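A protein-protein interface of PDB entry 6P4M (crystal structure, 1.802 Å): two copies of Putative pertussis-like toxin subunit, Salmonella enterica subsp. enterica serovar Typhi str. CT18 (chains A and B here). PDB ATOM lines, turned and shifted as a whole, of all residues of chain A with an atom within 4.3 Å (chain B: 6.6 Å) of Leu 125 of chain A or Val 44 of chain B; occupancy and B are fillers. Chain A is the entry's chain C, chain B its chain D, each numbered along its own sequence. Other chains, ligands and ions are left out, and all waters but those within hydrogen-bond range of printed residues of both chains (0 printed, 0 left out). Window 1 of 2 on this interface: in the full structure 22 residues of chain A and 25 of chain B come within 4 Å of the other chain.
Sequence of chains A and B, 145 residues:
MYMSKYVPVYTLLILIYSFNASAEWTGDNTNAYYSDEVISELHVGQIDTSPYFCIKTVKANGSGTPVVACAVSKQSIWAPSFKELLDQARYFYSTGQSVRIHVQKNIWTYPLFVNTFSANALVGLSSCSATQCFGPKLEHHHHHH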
ATOM      1  N   GLU A  84     -26.756  -0.122 -20.066  1.00  0.00           N
ATOM      2  CA  GLU A  84     -26.375   0.675 -18.904  1.00  0.00           C
ATOM      3  C   GLU A  84     -25.562   1.892 -19.321  1.00  0.00           C
ATOM      4  O   GLU A  84     -25.728   2.974 -18.750  1.00  0.00           O
ATOM      5  CB  GLU A  84     -25.589  -0.194 -17.918  1.00  0.00           C
ATOM      6  CG  GLU A  84     -26.448  -1.166 -17.117  1.00  0.00           C
ATOM      7  CD  GLU A  84     -26.791  -2.440 -17.872  1.00  0.00           C
ATOM      8  OE1 GLU A  84     -26.266  -2.656 -18.996  1.00  0.00           O
ATOM      9  OE2 GLU A  84     -27.605  -3.229 -17.333  1.00  0.00           O
ATOM     10  N   LEU A  85     -24.686   1.736 -20.325  1.00  0.00           N
ATOM     11  CA  LEU A  85     -23.881   2.860 -20.792  1.00  0.00           C
ATOM     12  C   LEU A  85     -24.719   3.860 -21.578  1.00  0.00           C
ATOM     13  O   LEU A  85     -24.460   5.065 -21.524  1.00  0.00           O
ATOM     14  CB  LEU A  85     -22.715   2.362 -21.652  1.00  0.00           C
ATOM     15  CG  LEU A  85     -21.556   1.681 -20.921  1.00  0.00           C
ATOM     16  CD1 LEU A  85     -20.580   1.060 -21.924  1.00  0.00           C
ATOM     17  CD2 LEU A  85     -20.830   2.652 -20.026  1.00  0.00           C
ATOM     18  N   GLN A  88     -26.529   5.807 -18.956  1.00  0.00           N
ATOM     19  CA  GLN A  88     -25.637   6.697 -18.218  1.00  0.00           C
ATOM     20  C   GLN A  88     -25.131   7.830 -19.095  1.00  0.00           C
ATOM     21  O   GLN A  88     -24.940   8.952 -18.615  1.00  0.00           O
ATOM     22  CB  GLN A  88     -24.452   5.920 -17.639  1.00  0.00           C
ATOM     23  CG  GLN A  88     -23.743   6.718 -16.551  1.00  0.00           C
ATOM     24  CD  GLN A  88     -24.707   7.076 -15.452  1.00  0.00           C
ATOM     25  OE1 GLN A  88     -25.429   6.207 -14.957  1.00  0.00           O
ATOM     26  NE2 GLN A  88     -24.753   8.361 -15.079  1.00  0.00           N
ATOM     27  N   ALA A  89     -24.867   7.551 -20.374  1.00  0.00           N
ATOM     28  CA  ALA A  89     -24.484   8.621 -21.283  1.00  0.00           C
ATOM     29  C   ALA A  89     -25.594   9.650 -21.385  1.00  0.00           C
ATOM     30  O   ALA A  89     -25.334  10.857 -21.375  1.00  0.00           O
ATOM     31  CB  ALA A  89     -24.146   8.061 -22.667  1.00  0.00           C
ATOM     32  N   PHE A  92     -25.595  11.837 -18.064  1.00  0.00           N
ATOM     33  CA  PHE A  92     -24.509  12.813 -18.030  1.00  0.00           C
ATOM     34  C   PHE A  92     -24.630  13.843 -19.156  1.00  0.00           C
ATOM     35  O   PHE A  92     -24.200  14.995 -18.995  1.00  0.00           O
ATOM     36  CB  PHE A  92     -23.168  12.088 -18.112  1.00  0.00           C
ATOM     37  CG  PHE A  92     -22.745  11.405 -16.825  1.00  0.00           C
ATOM     38  CD1 PHE A  92     -23.183  11.859 -15.585  1.00  0.00           C
ATOM     39  CD2 PHE A  92     -21.881  10.311 -16.867  1.00  0.00           C
ATOM     40  CE1 PHE A  92     -22.765  11.221 -14.402  1.00  0.00           C
ATOM     41  CE2 PHE A  92     -21.464   9.666 -15.698  1.00  0.00           C
ATOM     42  CZ  PHE A  92     -21.905  10.129 -14.461  1.00  0.00           C
ATOM     43  N   ARG A 100     -15.318  11.525 -16.552  1.00  0.00           N
ATOM     44  CA  ARG A 100     -14.214  10.785 -17.155  1.00  0.00           C
ATOM     45  C   ARG A 100     -14.801   9.739 -18.086  1.00  0.00           C
ATOM     46  O   ARG A 100     -15.678   8.962 -17.688  1.00  0.00           O
ATOM     47  CB  ARG A 100     -13.327  10.110 -16.103  1.00  0.00           C
ATOM     48  CG  ARG A 100     -12.262   9.182 -16.693  1.00  0.00           C
ATOM     49  CD  ARG A 100     -11.387   8.583 -15.604  1.00  0.00           C
ATOM     50  NE  ARG A 100     -10.545   9.611 -14.990  1.00  0.00           N
ATOM     51  CZ  ARG A 100      -9.686   9.373 -14.004  1.00  0.00           C
ATOM     52  NH1 ARG A 100      -9.554   8.142 -13.532  1.00  0.00           N
ATOM     53  NH2 ARG A 100      -8.954  10.365 -13.501  1.00  0.00           N
ATOM     54  N   ILE A 101     -14.360   9.750 -19.333  1.00  0.00           N
ATOM     55  CA  ILE A 101     -14.834   8.796 -20.323  1.00  0.00           C
ATOM     56  C   ILE A 101     -13.752   7.744 -20.504  1.00  0.00           C
ATOM     57  O   ILE A 101     -12.566   8.081 -20.619  1.00  0.00           O
ATOM     58  CB  ILE A 101     -15.190   9.496 -21.646  1.00  0.00           C
ATOM     59  CG1 ILE A 101     -15.482   8.468 -22.743  1.00  0.00           C
ATOM     60  CG2 ILE A 101     -14.102  10.456 -22.077  1.00  0.00           C
ATOM     61  CD1 ILE A 101     -16.121   9.082 -23.982  1.00  0.00           C
ATOM     62  N   HIS A 102     -14.146   6.475 -20.451  1.00  0.00           N
ATOM     63  CA  HIS A 102     -13.236   5.343 -20.590  1.00  0.00           C
ATOM     64  C   HIS A 102     -13.520   4.663 -21.915  1.00  0.00           C
ATOM     65  O   HIS A 102     -14.679   4.357 -22.209  1.00  0.00           O
ATOM     66  CB  HIS A 102     -13.423   4.335 -19.455  1.00  0.00           C
ATOM     67  CG  HIS A 102     -13.355   4.936 -18.084  1.00  0.00           C
ATOM     68  ND1 HIS A 102     -12.291   4.726 -17.233  1.00  0.00           N
ATOM     69  CD2 HIS A 102     -14.219   5.740 -17.415  1.00  0.00           C
ATOM     70  CE1 HIS A 102     -12.507   5.365 -16.093  1.00  0.00           C
ATOM     71  NE2 HIS A 102     -13.667   5.990 -16.180  1.00  0.00           N
ATOM     72  N   LEU A 122     -16.853   2.680 -26.232  1.00  0.00           N
ATOM     73  CA  LEU A 122     -17.093   3.250 -24.910  1.00  0.00           C
ATOM     74  C   LEU A 122     -17.178   2.121 -23.885  1.00  0.00           C
ATOM     75  O   LEU A 122     -17.932   1.160 -24.076  1.00  0.00           O
ATOM     76  CB  LEU A 122     -18.387   4.072 -24.928  1.00  0.00           C
ATOM     77  CG  LEU A 122     -18.787   4.658 -23.576  1.00  0.00           C
ATOM     78  CD1 LEU A 122     -17.808   5.739 -23.206  1.00  0.00           C
ATOM     79  CD2 LEU A 122     -20.205   5.211 -23.639  1.00  0.00           C
ATOM     80  N   GLY A 124     -16.808   2.865 -20.160  1.00  0.00           N
ATOM     81  CA  GLY A 124     -17.135   3.315 -18.818  1.00  0.00           C
ATOM     82  C   GLY A 124     -17.333   4.817 -18.784  1.00  0.00           C
ATOM     83  O   GLY A 124     -16.835   5.558 -19.643  1.00  0.00           O
ATOM     84  N   LEU A 125     -18.061   5.255 -17.751  1.00  0.00           N
ATOM     85  CA  LEU A 125     -18.307   6.673 -17.502  1.00  0.00           C
ATOM     86  C   LEU A 125     -18.248   6.916 -16.005  1.00  0.00           C
ATOM     87  O   LEU A 125     -18.873   6.180 -15.240  1.00  0.00           O
ATOM     88  CB  LEU A 125     -19.675   7.122 -18.043  1.00  0.00           C
ATOM     89  CG  LEU A 125     -19.790   7.115 -19.569  1.00  0.00           C
ATOM     90  CD1 LEU A 125     -21.264   7.193 -20.012  1.00  0.00           C
ATOM     91  CD2 LEU A 125     -18.970   8.248 -20.172  1.00  0.00           C
ATOM     92  N   SER A 126     -17.493   7.931 -15.594  1.00  0.00           N
ATOM     93  CA  SER A 126     -17.298   8.260 -14.182  1.00  0.00           C
ATOM     94  C   SER A 126     -17.634   9.722 -13.935  1.00  0.00           C
ATOM     95  O   SER A 126     -17.249  10.584 -14.723  1.00  0.00           O
ATOM     96  CB  SER A 126     -15.842   8.011 -13.755  1.00  0.00           C
ATOM     97  OG  SER A 126     -15.447   6.708 -14.107  1.00  0.00           O
ATOM     98  N   LEU B  42     -20.873   8.766  -9.033  1.00  0.00           N
ATOM     99  CA  LEU B  42     -21.461   7.606  -9.689  1.00  0.00           C
ATOM    100  C   LEU B  42     -20.573   7.188 -10.850  1.00  0.00           C
ATOM    101  O   LEU B  42     -20.130   8.037 -11.630  1.00  0.00           O
ATOM    102  CB  LEU B  42     -22.879   7.919 -10.198  1.00  0.00           C
ATOM    103  CG  LEU B  42     -23.575   6.906 -11.109  1.00  0.00           C
ATOM    104  CD1 LEU B  42     -23.811   5.605 -10.382  1.00  0.00           C
ATOM    105  CD2 LEU B  42     -24.896   7.496 -11.596  1.00  0.00           C
ATOM    106  N   HIS B  43     -20.336   5.880 -10.972  1.00  0.00           N
ATOM    107  CA  HIS B  43     -19.503   5.310 -12.029  1.00  0.00           C
ATOM    108  C   HIS B  43     -20.194   4.081 -12.598  1.00  0.00           C
ATOM    109  O   HIS B  43     -20.771   3.296 -11.847  1.00  0.00           O
ATOM    110  CB  HIS B  43     -18.103   4.922 -11.489  1.00  0.00           C
ATOM    111  CG  HIS B  43     -17.347   3.963 -12.363  1.00  0.00           C
ATOM    112  ND1 HIS B  43     -16.418   4.378 -13.293  1.00  0.00           N
ATOM    113  CD2 HIS B  43     -17.364   2.612 -12.428  1.00  0.00           C
ATOM    114  CE1 HIS B  43     -15.902   3.322 -13.901  1.00  0.00           C
ATOM    115  NE2 HIS B  43     -16.459   2.238 -13.395  1.00  0.00           N
ATOM    116  N   VAL B  44     -20.129   3.909 -13.922  1.00  0.00           N
ATOM    117  CA  VAL B  44     -20.691   2.743 -14.601  1.00  0.00           C
ATOM    118  C   VAL B  44     -19.606   2.119 -15.473  1.00  0.00           C
ATOM    119  O   VAL B  44     -18.900   2.831 -16.191  1.00  0.00           O
ATOM    120  CB  VAL B  44     -21.914   3.118 -15.464  1.00  0.00           C
ATOM    121  CG1 VAL B  44     -22.374   1.937 -16.282  1.00  0.00           C
ATOM    122  CG2 VAL B  44     -23.060   3.601 -14.576  1.00  0.00           C
ATOM    123  N   GLY B  45     -19.480   0.801 -15.417  1.00  0.00           N
ATOM    124  CA  GLY B  45     -18.513   0.119 -16.253  1.00  0.00           C
ATOM    125  C   GLY B  45     -18.883  -1.328 -16.474  1.00  0.00           C
ATOM    126  O   GLY B  45     -20.034  -1.730 -16.295  1.00  0.00           O
ATOM    127  N   GLN B  46     -17.887  -2.122 -16.875  1.00  0.00           N
ATOM    128  CA  GLN B  46     -18.081  -3.550 -17.091  1.00  0.00           C
ATOM    129  C   GLN B  46     -16.900  -4.325 -16.518  1.00  0.00           C
ATOM    130  O   GLN B  46     -15.759  -3.860 -16.594  1.00  0.00           O
ATOM    131  CB  GLN B  46     -18.229  -3.878 -18.585  1.00  0.00           C
ATOM    132  CG  GLN B  46     -18.576  -5.336 -18.860  1.00  0.00           C
ATOM    133  CD  GLN B  46     -18.768  -5.612 -20.335  1.00  0.00           C
ATOM    134  OE1 GLN B  46     -19.670  -5.061 -20.963  1.00  0.00           O
ATOM    135  NE2 GLN B  46     -17.910  -6.466 -20.905  1.00  0.00           N
ATOM    136  N   PRO B  51     -22.119  -5.745 -16.545  1.00  0.00           N
ATOM    137  CA  PRO B  51     -22.217  -4.333 -16.158  1.00  0.00           C
ATOM    138  C   PRO B  51     -22.137  -4.221 -14.644  1.00  0.00           C
ATOM    139  O   PRO B  51     -22.526  -5.133 -13.911  1.00  0.00           O
ATOM    140  CB  PRO B  51     -23.587  -3.885 -16.690  1.00  0.00           C
ATOM    141  CG  PRO B  51     -24.307  -5.117 -17.108  1.00  0.00           C
ATOM    142  CD  PRO B  51     -23.351  -6.275 -17.157  1.00  0.00           C
ATOM    143  N   TYR B  52     -21.593  -3.105 -14.180  1.00  0.00           N
ATOM    144  CA  TYR B  52     -21.575  -2.830 -12.749  1.00  0.00           C
ATOM    145  C   TYR B  52     -21.673  -1.327 -12.558  1.00  0.00           C
ATOM    146  O   TYR B  52     -21.421  -0.549 -13.483  1.00  0.00           O
ATOM    147  CB  TYR B  52     -20.305  -3.406 -12.081  1.00  0.00           C
ATOM    148  CG  TYR B  52     -19.050  -2.614 -12.392  1.00  0.00           C
ATOM    149  CD1 TYR B  52     -18.273  -2.912 -13.498  1.00  0.00           C
ATOM    150  CD2 TYR B  52     -18.651  -1.555 -11.586  1.00  0.00           C
ATOM    151  CE1 TYR B  52     -17.132  -2.170 -13.805  1.00  0.00           C
ATOM    152  CE2 TYR B  52     -17.520  -0.805 -11.885  1.00  0.00           C
ATOM    153  CZ  TYR B  52     -16.756  -1.133 -12.993  1.00  0.00           C
ATOM    154  OH  TYR B  52     -15.641  -0.391 -13.297  1.00  0.00           O
ATOM    155  N   PHE B  53     -22.045  -0.908 -11.348  1.00  0.00           N
ATOM    156  CA  PHE B  53     -21.908   0.495 -11.007  1.00  0.00           C
ATOM    157  C   PHE B  53     -21.390   0.616  -9.583  1.00  0.00           C
ATOM    158  O   PHE B  53     -21.503  -0.308  -8.774  1.00  0.00           O
ATOM    159  CB  PHE B  53     -23.228   1.285 -11.182  1.00  0.00           C
ATOM    160  CG  PHE B  53     -24.246   1.057 -10.093  1.00  0.00           C
ATOM    161  CD1 PHE B  53     -25.134   0.000 -10.162  1.00  0.00           C
ATOM    162  CD2 PHE B  53     -24.347   1.938  -9.020  1.00  0.00           C
ATOM    163  CE1 PHE B  53     -26.079  -0.194  -9.165  1.00  0.00           C
ATOM    164  CE2 PHE B  53     -25.287   1.741  -8.026  1.00  0.00           C
ATOM    165  CZ  PHE B  53     -26.154   0.687  -8.097  1.00  0.00           C
ATOM    166  N   CYS B  54     -20.825   1.783  -9.298  1.00  0.00           N
ATOM    167  CA  CYS B  54     -20.332   2.129  -7.975  1.00  0.00           C
ATOM    168  C   CYS B  54     -20.830   3.511  -7.608  1.00  0.00           C
ATOM    169  O   CYS B  54     -21.003   4.367  -8.474  1.00  0.00           O
ATOM    170  CB  CYS B  54     -18.809   2.117  -7.929  1.00  0.00           C
ATOM    171  SG  CYS B  54     -18.118   0.508  -8.341  1.00  0.00           S
ATOM    172  N   PHE B  82     -29.866  -5.611  -9.124  1.00  0.00           N
ATOM    173  CA  PHE B  82     -28.960  -4.667  -9.785  1.00  0.00           C
ATOM    174  C   PHE B  82     -29.711  -3.499 -10.421  1.00  0.00           C
ATOM    175  O   PHE B  82     -29.381  -2.331 -10.192  1.00  0.00           O
ATOM    176  CB  PHE B  82     -28.130  -5.395 -10.852  1.00  0.00           C
ATOM    177  CG  PHE B  82     -27.236  -4.483 -11.656  1.00  0.00           C
ATOM    178  CD1 PHE B  82     -26.006  -4.082 -11.155  1.00  0.00           C
ATOM    179  CD2 PHE B  82     -27.618  -4.036 -12.916  1.00  0.00           C
ATOM    180  CE1 PHE B  82     -25.190  -3.236 -11.868  1.00  0.00           C
ATOM    181  CE2 PHE B  82     -26.787  -3.185 -13.647  1.00  0.00           C
ATOM    182  CZ  PHE B  82     -25.577  -2.785 -13.121  1.00  0.00           C
ATOM    183  N   LEU B  86     -29.583   0.406  -9.280  1.00  0.00           N
ATOM    184  CA  LEU B  86     -29.000   1.415 -10.155  1.00  0.00           C
ATOM    185  C   LEU B  86     -29.997   2.531 -10.405  1.00  0.00           C
ATOM    186  O   LEU B  86     -29.641   3.714 -10.367  1.00  0.00           O
ATOM    187  CB  LEU B  86     -28.538   0.789 -11.476  1.00  0.00           C
ATOM    188  CG  LEU B  86     -28.110   1.749 -12.596  1.00  0.00           C
ATOM    189  CD1 LEU B  86     -26.956   2.635 -12.138  1.00  0.00           C
ATOM    190  CD2 LEU B  86     -27.707   0.978 -13.861  1.00  0.00           C
ATOM    191  N   ARG B  90     -29.417   6.394  -9.100  1.00  0.00           N
ATOM    192  CA  ARG B  90     -29.449   7.529 -10.013  1.00  0.00           C
ATOM    193  C   ARG B  90     -30.427   8.586  -9.533  1.00  0.00           C
ATOM    194  O   ARG B  90     -30.149   9.785  -9.619  1.00  0.00           O
ATOM    195  CB  ARG B  90     -29.836   7.062 -11.413  1.00  0.00           C
ATOM    196  CG  ARG B  90     -28.689   6.509 -12.227  1.00  0.00           C
ATOM    197  CD  ARG B  90     -29.234   5.951 -13.534  1.00  0.00           C
ATOM    198  NE  ARG B  90     -28.156   5.440 -14.372  1.00  0.00           N
ATOM    199  CZ  ARG B  90     -28.293   4.414 -15.198  1.00  0.00           C
ATOM    200  NH1 ARG B  90     -29.459   3.798 -15.289  1.00  0.00           N
ATOM    201  NH2 ARG B  90     -27.265   4.010 -15.932  1.00  0.00           N
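OE1 of Glu 84 of chain A touches CG of Pro 51 of chain B, 3.7 Å away. Glu 84 of chain A touches Phe 82 of chain B. Leu 42 of chain B touches Gln 88 of chain A (CD2 to NE2, 3.6 Å). OE1 of Gln 88 of chain A touches CG2 of Val 44 of chain B, 3.5 Å away. Leu 42 of chain B touches Phe 92 of chain A. Gly 124 of chain A touches Val 44 of chain B (CA to O, 3.2 Å). Leu 125 of chain A touches His 43 of chain B. O of Leu 42 of chain B touches C of Ser 126 of chain A, 3.8 Å away.
The side-chain hydroxyl (OG) of Ser 126 of chain A is in hydrogen-bond range of a ring nitrogen (ND1) of His 43 of chain B (2.7 Å). The backbone carbonyl oxygen (O) of Leu 125 of chain A is in hydrogen-bond range of the backbone NH (N) of Val 44 of chain B, 2.9 Å away. O of Glu 84 of chain A sits at hydrogen-bond distance from NH2 of Arg 90 of chain B. OE1 of Gln 88 of chain A is in hydrogen-bond range of NE of Arg 90 of chain B.
No position is printed for both chains. Of the 12 pairs that touch across the chains among the printed residues, none has its exchanged pair printed and touching as well.
Printed residues of chain A that touch a printed residue of chain B: Glu 84, Gln 88, Phe 92, Gly 124, Leu 125 and Ser 126. Of the 12 printed residues of chain B, 6 touch a printed residue of chain A. Printed residues of chain B that touch a printed residue of chain A: Leu 42, His 43, Val 44, Pro 51, Phe 82 and Arg 90. Among the printed residues, no Asp or Glu carboxylate lies within 4 Å of a Lys or Arg side-chain nitrogen of the other chain.
Of chain A, only Gln 88 (3.5 Å), Gly 124 (3.2 Å) and Leu 125 (2.9 Å) come within 4 Å of Val 44 of chain B. Of the printed residues of chain A, Phe 82 of chain B touches Glu 84 (3.8 Å). Printed residues of chain B within 4 Å of Gly 124 of chain A: Val 44 (3.2 Å). Printed residues of chain B within 4 Å of Gln 88 of chain A: Leu 42 (3.6 Å), Val 44 (3.5 Å) and Arg 90 (2.9 Å). Printed residues of chain A within 4 Å of Pro 51 of chain B: Glu 84 (3.7 Å). Printed residues of chain A within 4 Å of Arg 90 of chain B: Glu 84 and Gln 88. Arg 100 of chain A touches none of the printed residues of chain B. Ala 89 of chain A touches none of the printed residues of chain B. The nearest residue of chain B that does not touch Leu 125 of chain A is Leu 42 of chain B (4.2 Å).
O of Gly 124 of chain A sits at hydrogen-bond distance from N of His 102 of chain A. The backbone NH of Arg 100 of chain A sits at hydrogen-bond distance from the backbone carbonyl oxygen of Ser 126 of chain A, at 2.8 Å. A ring nitrogen (NE2) of His 102 of chain A sits at hydrogen-bond distance from the side-chain hydroxyl (OG) of Ser 126 of chain A (2.8 Å). O of His 43 of chain B lies within hydrogen-bond range of N of Cys 54 of chain B, 3.0 Å away. NE2 of His 43 of chain B sits at hydrogen-bond distance from OH of Tyr 52 of chain B.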
